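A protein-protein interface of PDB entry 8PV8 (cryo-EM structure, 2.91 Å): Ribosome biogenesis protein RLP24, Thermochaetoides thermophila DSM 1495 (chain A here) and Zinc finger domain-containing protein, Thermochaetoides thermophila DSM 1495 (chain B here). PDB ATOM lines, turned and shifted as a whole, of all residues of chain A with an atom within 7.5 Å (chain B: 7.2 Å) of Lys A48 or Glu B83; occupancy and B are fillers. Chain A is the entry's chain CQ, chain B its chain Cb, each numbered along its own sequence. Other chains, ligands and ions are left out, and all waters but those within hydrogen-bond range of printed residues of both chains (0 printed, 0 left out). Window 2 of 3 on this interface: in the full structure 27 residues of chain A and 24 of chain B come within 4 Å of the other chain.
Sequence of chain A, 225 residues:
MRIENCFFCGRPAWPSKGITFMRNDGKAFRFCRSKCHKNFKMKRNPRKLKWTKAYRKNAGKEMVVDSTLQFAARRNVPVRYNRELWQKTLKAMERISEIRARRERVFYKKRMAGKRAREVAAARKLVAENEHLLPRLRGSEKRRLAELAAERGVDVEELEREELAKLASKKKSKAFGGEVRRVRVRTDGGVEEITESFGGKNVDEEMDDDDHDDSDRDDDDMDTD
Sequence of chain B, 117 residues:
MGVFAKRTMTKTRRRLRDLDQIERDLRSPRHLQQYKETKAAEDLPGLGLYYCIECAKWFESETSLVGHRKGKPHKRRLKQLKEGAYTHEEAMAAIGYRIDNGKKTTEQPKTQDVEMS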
ATOM      1  N   ARG A  44     -11.238   4.822  -9.526  1.00  0.00           N
ATOM      2  CA  ARG A  44     -11.312   3.642 -10.372  1.00  0.00           C
ATOM      3  C   ARG A  44     -10.686   3.953 -11.723  1.00  0.00           C
ATOM      4  O   ARG A  44     -10.867   5.045 -12.269  1.00  0.00           O
ATOM      5  CB  ARG A  44     -12.761   3.193 -10.553  1.00  0.00           C
ATOM      6  CG  ARG A  44     -13.518   2.986  -9.254  1.00  0.00           C
ATOM      7  CD  ARG A  44     -14.494   1.830  -9.374  1.00  0.00           C
ATOM      8  NE  ARG A  44     -13.808   0.562  -9.586  1.00  0.00           N
ATOM      9  CZ  ARG A  44     -14.420  -0.598  -9.779  1.00  0.00           C
ATOM     10  NH1 ARG A  44     -15.739  -0.686  -9.808  1.00  0.00           N
ATOM     11  NH2 ARG A  44     -13.691  -1.695  -9.949  1.00  0.00           N
ATOM     12  N   ASN A  45      -9.945   2.992 -12.254  1.00  0.00           N
ATOM     13  CA  ASN A  45      -9.269   3.198 -13.529  1.00  0.00           C
ATOM     14  C   ASN A  45     -10.269   3.058 -14.672  1.00  0.00           C
ATOM     15  O   ASN A  45     -10.974   2.048 -14.747  1.00  0.00           O
ATOM     16  CB  ASN A  45      -8.130   2.197 -13.697  1.00  0.00           C
ATOM     17  CG  ASN A  45      -7.065   2.677 -14.665  1.00  0.00           C
ATOM     18  OD1 ASN A  45      -7.367   3.152 -15.757  1.00  0.00           O
ATOM     19  ND2 ASN A  45      -5.807   2.551 -14.264  1.00  0.00           N
ATOM     20  N   PRO A  46     -10.376   4.056 -15.557  1.00  0.00           N
ATOM     21  CA  PRO A  46     -11.252   3.906 -16.733  1.00  0.00           C
ATOM     22  C   PRO A  46     -10.824   2.792 -17.668  1.00  0.00           C
ATOM     23  O   PRO A  46     -11.671   2.215 -18.360  1.00  0.00           O
ATOM     24  CB  PRO A  46     -11.162   5.277 -17.418  1.00  0.00           C
ATOM     25  CG  PRO A  46     -10.647   6.204 -16.380  1.00  0.00           C
ATOM     26  CD  PRO A  46      -9.772   5.396 -15.482  1.00  0.00           C
ATOM     27  N   ARG A  47      -9.529   2.470 -17.707  1.00  0.00           N
ATOM     28  CA  ARG A  47      -9.022   1.411 -18.570  1.00  0.00           C
ATOM     29  C   ARG A  47      -9.455   0.021 -18.117  1.00  0.00           C
ATOM     30  O   ARG A  47      -9.321  -0.931 -18.893  1.00  0.00           O
ATOM     31  CB  ARG A  47      -7.496   1.490 -18.633  1.00  0.00           C
ATOM     32  CG  ARG A  47      -6.888   0.972 -19.926  1.00  0.00           C
ATOM     33  CD  ARG A  47      -5.372   0.872 -19.837  1.00  0.00           C
ATOM     34  NE  ARG A  47      -4.743   2.146 -19.511  1.00  0.00           N
ATOM     35  CZ  ARG A  47      -4.128   2.407 -18.366  1.00  0.00           C
ATOM     36  NH1 ARG A  47      -4.040   1.502 -17.406  1.00  0.00           N
ATOM     37  NH2 ARG A  47      -3.584   3.607 -18.180  1.00  0.00           N
ATOM     38  N   LYS A  48      -9.971  -0.120 -16.895  1.00  0.00           N
ATOM     39  CA  LYS A  48     -10.432  -1.407 -16.396  1.00  0.00           C
ATOM     40  C   LYS A  48     -11.945  -1.531 -16.319  1.00  0.00           C
ATOM     41  O   LYS A  48     -12.449  -2.656 -16.240  1.00  0.00           O
ATOM     42  CB  LYS A  48      -9.834  -1.685 -15.010  1.00  0.00           C
ATOM     43  CG  LYS A  48      -8.331  -1.899 -15.032  1.00  0.00           C
ATOM     44  CD  LYS A  48      -7.893  -2.894 -13.974  1.00  0.00           C
ATOM     45  CE  LYS A  48      -6.466  -3.354 -14.215  1.00  0.00           C
ATOM     46  NZ  LYS A  48      -6.050  -4.411 -13.254  1.00  0.00           N
ATOM     47  N   LEU A  49     -12.679  -0.421 -16.338  1.00  0.00           N
ATOM     48  CA  LEU A  49     -14.135  -0.466 -16.377  1.00  0.00           C
ATOM     49  C   LEU A  49     -14.586  -0.652 -17.821  1.00  0.00           C
ATOM     50  O   LEU A  49     -14.261   0.166 -18.688  1.00  0.00           O
ATOM     51  CB  LEU A  49     -14.727   0.804 -15.771  1.00  0.00           C
ATOM     52  CG  LEU A  49     -14.239   1.140 -14.359  1.00  0.00           C
ATOM     53  CD1 LEU A  49     -14.927   2.381 -13.822  1.00  0.00           C
ATOM     54  CD2 LEU A  49     -14.457  -0.036 -13.423  1.00  0.00           C
ATOM     55  N   LYS A  50     -15.350  -1.716 -18.074  1.00  0.00           N
ATOM     56  CA  LYS A  50     -15.584  -2.179 -19.437  1.00  0.00           C
ATOM     57  C   LYS A  50     -16.590  -1.339 -20.211  1.00  0.00           C
ATOM     58  O   LYS A  50     -16.764  -1.573 -21.411  1.00  0.00           O
ATOM     59  CB  LYS A  50     -16.030  -3.641 -19.423  1.00  0.00           C
ATOM     60  CG  LYS A  50     -15.111  -4.542 -18.620  1.00  0.00           C
ATOM     61  CD  LYS A  50     -15.574  -5.985 -18.652  1.00  0.00           C
ATOM     62  CE  LYS A  50     -14.548  -6.895 -18.002  1.00  0.00           C
ATOM     63  NZ  LYS A  50     -14.934  -8.328 -18.103  1.00  0.00           N
ATOM     64  N   TRP A  51     -17.250  -0.380 -19.573  1.00  0.00           N
ATOM     65  CA  TRP A  51     -18.177   0.505 -20.264  1.00  0.00           C
ATOM     66  C   TRP A  51     -17.511   1.781 -20.759  1.00  0.00           C
ATOM     67  O   TRP A  51     -18.209   2.697 -21.203  1.00  0.00           O
ATOM     68  CB  TRP A  51     -19.358   0.851 -19.354  1.00  0.00           C
ATOM     69  CG  TRP A  51     -18.960   1.318 -17.990  1.00  0.00           C
ATOM     70  CD1 TRP A  51     -18.707   0.540 -16.900  1.00  0.00           C
ATOM     71  CD2 TRP A  51     -18.763   2.672 -17.568  1.00  0.00           C
ATOM     72  NE1 TRP A  51     -18.369   1.323 -15.827  1.00  0.00           N
ATOM     73  CE2 TRP A  51     -18.395   2.637 -16.211  1.00  0.00           C
ATOM     74  CE3 TRP A  51     -18.863   3.911 -18.208  1.00  0.00           C
ATOM     75  CZ2 TRP A  51     -18.126   3.790 -15.481  1.00  0.00           C
ATOM     76  CZ3 TRP A  51     -18.596   5.055 -17.480  1.00  0.00           C
ATOM     77  CH2 TRP A  51     -18.232   4.987 -16.132  1.00  0.00           C
ATOM     78  N   THR A  52     -16.186   1.860 -20.700  1.00  0.00           N
ATOM     79  CA  THR A  52     -15.455   3.062 -21.065  1.00  0.00           C
ATOM     80  C   THR A  52     -14.712   2.876 -22.382  1.00  0.00           C
ATOM     81  O   THR A  52     -14.173   1.800 -22.678  1.00  0.00           O
ATOM     82  CB  THR A  52     -14.459   3.459 -19.973  1.00  0.00           C
ATOM     83  OG1 THR A  52     -13.498   2.412 -19.798  1.00  0.00           O
ATOM     84  CG2 THR A  52     -15.181   3.707 -18.659  1.00  0.00           C
ATOM     85  N   ALA A  54     -11.919   4.084 -23.032  1.00  0.00           N
ATOM     86  CA  ALA A  54     -10.539   3.745 -22.703  1.00  0.00           C
ATOM     87  C   ALA A  54     -10.327   2.237 -22.695  1.00  0.00           C
ATOM     88  O   ALA A  54      -9.364   1.733 -23.288  1.00  0.00           O
ATOM     89  CB  ALA A  54     -10.166   4.345 -21.350  1.00  0.00           C
ATOM     90  N   TYR A  55     -11.229   1.498 -22.041  1.00  0.00           N
ATOM     91  CA  TYR A  55     -11.128   0.043 -22.034  1.00  0.00           C
ATOM     92  C   TYR A  55     -11.321  -0.528 -23.429  1.00  0.00           C
ATOM     93  O   TYR A  55     -10.639  -1.485 -23.810  1.00  0.00           O
ATOM     94  CB  TYR A  55     -12.149  -0.570 -21.073  1.00  0.00           C
ATOM     95  CG  TYR A  55     -12.252  -2.086 -21.160  1.00  0.00           C
ATOM     96  CD1 TYR A  55     -13.216  -2.706 -21.957  1.00  0.00           C
ATOM     97  CD2 TYR A  55     -11.383  -2.897 -20.444  1.00  0.00           C
ATOM     98  CE1 TYR A  55     -13.303  -4.080 -22.036  1.00  0.00           C
ATOM     99  CE2 TYR A  55     -11.465  -4.274 -20.518  1.00  0.00           C
ATOM    100  CZ  TYR A  55     -12.426  -4.858 -21.314  1.00  0.00           C
ATOM    101  OH  TYR A  55     -12.513  -6.227 -21.389  1.00  0.00           O
ATOM    102  N   ASN A  58      -8.204   0.046 -25.370  1.00  0.00           N
ATOM    103  CA  ASN A  58      -7.128  -0.803 -24.870  1.00  0.00           C
ATOM    104  C   ASN A  58      -7.308  -2.253 -25.298  1.00  0.00           C
ATOM    105  O   ASN A  58      -6.321  -2.938 -25.590  1.00  0.00           O
ATOM    106  CB  ASN A  58      -7.051  -0.704 -23.348  1.00  0.00           C
ATOM    107  CG  ASN A  58      -5.842  -1.415 -22.781  1.00  0.00           C
ATOM    108  OD1 ASN A  58      -4.768  -1.411 -23.380  1.00  0.00           O
ATOM    109  ND2 ASN A  58      -6.011  -2.034 -21.618  1.00  0.00           N
ATOM    110  N   ARG B  77       0.151  -0.353  -5.496  1.00  0.00           N
ATOM    111  CA  ARG B  77       0.610   0.905  -6.079  1.00  0.00           C
ATOM    112  C   ARG B  77       1.692   0.668  -7.127  1.00  0.00           C
ATOM    113  O   ARG B  77       1.696   1.319  -8.181  1.00  0.00           O
ATOM    114  CB  ARG B  77       1.110   1.838  -4.979  1.00  0.00           C
ATOM    115  CG  ARG B  77       0.006   2.670  -4.352  1.00  0.00           C
ATOM    116  CD  ARG B  77      -0.577   3.643  -5.361  1.00  0.00           C
ATOM    117  NE  ARG B  77      -1.805   4.269  -4.885  1.00  0.00           N
ATOM    118  CZ  ARG B  77      -1.850   5.341  -4.108  1.00  0.00           C
ATOM    119  NH1 ARG B  77      -0.747   5.928  -3.676  1.00  0.00           N
ATOM    120  NH2 ARG B  77      -3.032   5.838  -3.754  1.00  0.00           N
ATOM    121  N   LEU B  78       2.601  -0.277  -6.866  1.00  0.00           N
ATOM    122  CA  LEU B  78       3.632  -0.615  -7.844  1.00  0.00           C
ATOM    123  C   LEU B  78       3.032  -1.189  -9.123  1.00  0.00           C
ATOM    124  O   LEU B  78       3.461  -0.837 -10.226  1.00  0.00           O
ATOM    125  CB  LEU B  78       4.634  -1.600  -7.244  1.00  0.00           C
ATOM    126  CG  LEU B  78       5.593  -1.067  -6.182  1.00  0.00           C
ATOM    127  CD1 LEU B  78       6.542  -2.165  -5.734  1.00  0.00           C
ATOM    128  CD2 LEU B  78       6.363   0.129  -6.709  1.00  0.00           C
ATOM    129  N   LYS B  79       2.037  -2.071  -8.998  1.00  0.00           N
ATOM    130  CA  LYS B  79       1.429  -2.666 -10.186  1.00  0.00           C
ATOM    131  C   LYS B  79       0.605  -1.642 -10.962  1.00  0.00           C
ATOM    132  O   LYS B  79       0.581  -1.666 -12.199  1.00  0.00           O
ATOM    133  CB  LYS B  79       0.574  -3.870  -9.793  1.00  0.00           C
ATOM    134  CG  LYS B  79      -0.011  -4.623 -10.976  1.00  0.00           C
ATOM    135  CD  LYS B  79      -0.778  -5.854 -10.535  1.00  0.00           C
ATOM    136  CE  LYS B  79      -1.357  -6.587 -11.733  1.00  0.00           C
ATOM    137  NZ  LYS B  79      -2.116  -7.800 -11.329  1.00  0.00           N
ATOM    138  N   GLN B  80      -0.069  -0.732 -10.254  1.00  0.00           N
ATOM    139  CA  GLN B  80      -0.799   0.342 -10.923  1.00  0.00           C
ATOM    140  C   GLN B  80       0.147   1.278 -11.667  1.00  0.00           C
ATOM    141  O   GLN B  80      -0.164   1.726 -12.776  1.00  0.00           O
ATOM    142  CB  GLN B  80      -1.637   1.121  -9.910  1.00  0.00           C
ATOM    143  CG  GLN B  80      -2.852   0.367  -9.400  1.00  0.00           C
ATOM    144  CD  GLN B  80      -3.624   1.144  -8.355  1.00  0.00           C
ATOM    145  OE1 GLN B  80      -3.213   2.226  -7.939  1.00  0.00           O
ATOM    146  NE2 GLN B  80      -4.755   0.597  -7.929  1.00  0.00           N
ATOM    147  N   LEU B  81       1.306   1.579 -11.077  1.00  0.00           N
ATOM    148  CA  LEU B  81       2.294   2.395 -11.776  1.00  0.00           C
ATOM    149  C   LEU B  81       2.922   1.647 -12.945  1.00  0.00           C
ATOM    150  O   LEU B  81       3.291   2.269 -13.949  1.00  0.00           O
ATOM    151  CB  LEU B  81       3.372   2.859 -10.801  1.00  0.00           C
ATOM    152  CG  LEU B  81       2.932   3.932  -9.808  1.00  0.00           C
ATOM    153  CD1 LEU B  81       3.861   3.947  -8.614  1.00  0.00           C
ATOM    154  CD2 LEU B  81       2.891   5.294 -10.475  1.00  0.00           C
ATOM    155  N   LYS B  82       3.070   0.325 -12.827  1.00  0.00           N
ATOM    156  CA  LYS B  82       3.582  -0.478 -13.932  1.00  0.00           C
ATOM    157  C   LYS B  82       2.610  -0.483 -15.105  1.00  0.00           C
ATOM    158  O   LYS B  82       3.023  -0.382 -16.267  1.00  0.00           O
ATOM    159  CB  LYS B  82       3.854  -1.905 -13.456  1.00  0.00           C
ATOM    160  CG  LYS B  82       4.523  -2.789 -14.491  1.00  0.00           C
ATOM    161  CD  LYS B  82       4.764  -4.183 -13.944  1.00  0.00           C
ATOM    162  CE  LYS B  82       5.861  -4.180 -12.895  1.00  0.00           C
ATOM    163  NZ  LYS B  82       7.187  -3.853 -13.483  1.00  0.00           N
ATOM    164  N   GLU B  83       1.313  -0.612 -14.819  1.00  0.00           N
ATOM    165  CA  GLU B  83       0.312  -0.525 -15.880  1.00  0.00           C
ATOM    166  C   GLU B  83       0.238   0.886 -16.451  1.00  0.00           C
ATOM    167  O   GLU B  83       0.006   1.066 -17.652  1.00  0.00           O
ATOM    168  CB  GLU B  83      -1.056  -0.965 -15.359  1.00  0.00           C
ATOM    169  CG  GLU B  83      -1.143  -2.437 -15.001  1.00  0.00           C
ATOM    170  CD  GLU B  83      -2.510  -2.826 -14.474  1.00  0.00           C
ATOM    171  OE1 GLU B  83      -3.347  -1.923 -14.270  1.00  0.00           O
ATOM    172  OE2 GLU B  83      -2.749  -4.034 -14.267  1.00  0.00           O
ATOM    173  N   GLY B  84       0.434   1.896 -15.608  1.00  0.00           N
ATOM    174  CA  GLY B  84       0.418   3.271 -16.058  1.00  0.00           C
ATOM    175  C   GLY B  84      -0.825   4.020 -15.628  1.00  0.00           C
ATOM    176  O   GLY B  84      -1.929   3.468 -15.650  1.00  0.00           O
ATOM    177  N   ALA B  85      -0.656   5.276 -15.228  1.00  0.00           N
ATOM    178  CA  ALA B  85      -1.791   6.089 -14.832  1.00  0.00           C
ATOM    179  C   ALA B  85      -2.586   6.534 -16.056  1.00  0.00           C
ATOM    180  O   ALA B  85      -2.062   6.651 -17.167  1.00  0.00           O
ATOM    181  CB  ALA B  85      -1.329   7.309 -14.037  1.00  0.00           C
ATOM    182  N   TYR B  86      -3.872   6.783 -15.837  1.00  0.00           N
ATOM    183  CA  TYR B  86      -4.760   7.250 -16.890  1.00  0.00           C
ATOM    184  C   TYR B  86      -4.651   8.764 -17.002  1.00  0.00           C
ATOM    185  O   TYR B  86      -4.817   9.479 -16.009  1.00  0.00           O
ATOM    186  CB  TYR B  86      -6.200   6.833 -16.596  1.00  0.00           C
ATOM    187  CG  TYR B  86      -7.179   7.225 -17.670  1.00  0.00           C
ATOM    188  CD1 TYR B  86      -7.277   6.495 -18.845  1.00  0.00           C
ATOM    189  CD2 TYR B  86      -8.012   8.322 -17.506  1.00  0.00           C
ATOM    190  CE1 TYR B  86      -8.172   6.849 -19.827  1.00  0.00           C
ATOM    191  CE2 TYR B  86      -8.913   8.682 -18.482  1.00  0.00           C
ATOM    192  CZ  TYR B  86      -8.989   7.941 -19.641  1.00  0.00           C
ATOM    193  OH  TYR B  86      -9.886   8.291 -20.622  1.00  0.00           O
ATOM    194  N   GLU B  90      -4.067   9.725 -22.959  1.00  0.00           N
ATOM    195  CA  GLU B  90      -4.714   8.432 -23.139  1.00  0.00           C
ATOM    196  C   GLU B  90      -6.205   8.593 -23.414  1.00  0.00           C
ATOM    197  O   GLU B  90      -6.777   7.816 -24.185  1.00  0.00           O
ATOM    198  CB  GLU B  90      -4.481   7.549 -21.914  1.00  0.00           C
ATOM    199  CG  GLU B  90      -5.047   6.145 -22.046  1.00  0.00           C
ATOM    200  CD  GLU B  90      -4.754   5.283 -20.840  1.00  0.00           C
ATOM    201  OE1 GLU B  90      -4.127   5.790 -19.888  1.00  0.00           O
ATOM    202  OE2 GLU B  90      -5.139   4.095 -20.851  1.00  0.00           O
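Lys A48 touches just one residue of chain B: Glu B83. Of the printed residues of chain A, Glu B90 touches Arg A47. Of the printed residues of chain A, Tyr B86 touches Asn A45, Pro A46, Arg A47 and Ala A54. Of the printed residues of chain A, Gly B84 touches Arg A47 (3.0 Å). Of the printed residues of chain B, Pro A46 touches Tyr B86. Of the printed residues of chain B, Arg A47 touches Gly B84, Ala B85, Tyr B86 and Glu B90. Gln B80 touches none of the printed residues of chain A. Arg B77 touches none of the printed residues of chain A. The nearest residue of chain B that does not touch Lys A48 is Lys B79 (5.4 Å). The nearest residue of chain A that does not touch Glu B83 is Arg A47 (4.1 Å). The nearest printed residue of chain B that does not touch Ala A54 is Glu B90 (5.1 Å).
OD1 of Asn A45 sits at hydrogen-bond distance from N of Arg A47.
Among the printed residues, merely in contact across the chains: Asn A45 with Tyr B86 (3.95 Å), Pro A46 with Tyr B86 (3.6 Å), Arg A47 with Ala B85 (3.6 Å), Arg A47 with Tyr B86 (3.96 Å) and Ala A54 with Tyr B86 (3.5 Å).
Hydrophobic or aromatic side chains of chain B within 4 Å of the printed part of chain A: Tyr B86. Along chain B the printed residues that touch a printed residue of chain A span positions 83 to 90. Of the 12 printed residues of chain A, 5 touch a printed residue of chain B. Hydrophobic or aromatic side chains of chain A that line the printed part of chain B: Pro A46 and Ala A54. Among the printed residues, 8 pairs touch across the chains. Among the printed residues, Asp or Glu carboxylates within 4 Å of a Lys or Arg side-chain nitrogen of the other chain: Arg A47 with Glu B90 (2.4 Å) and Lys A48 with Glu B83 (3.5 Å).
The side-chain amino group (NZ) of Lys A48 is in salt-bridge range of the side-chain carboxylate (OE2) of Glu B83 (3.5 Å). O of Gly B84 is in hydrogen-bond range of NH2 of Arg A47 (3.0 Å). NH2 of Arg A47 lies within salt-bridge range of OE1 of Glu B90 (2.8 Å).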
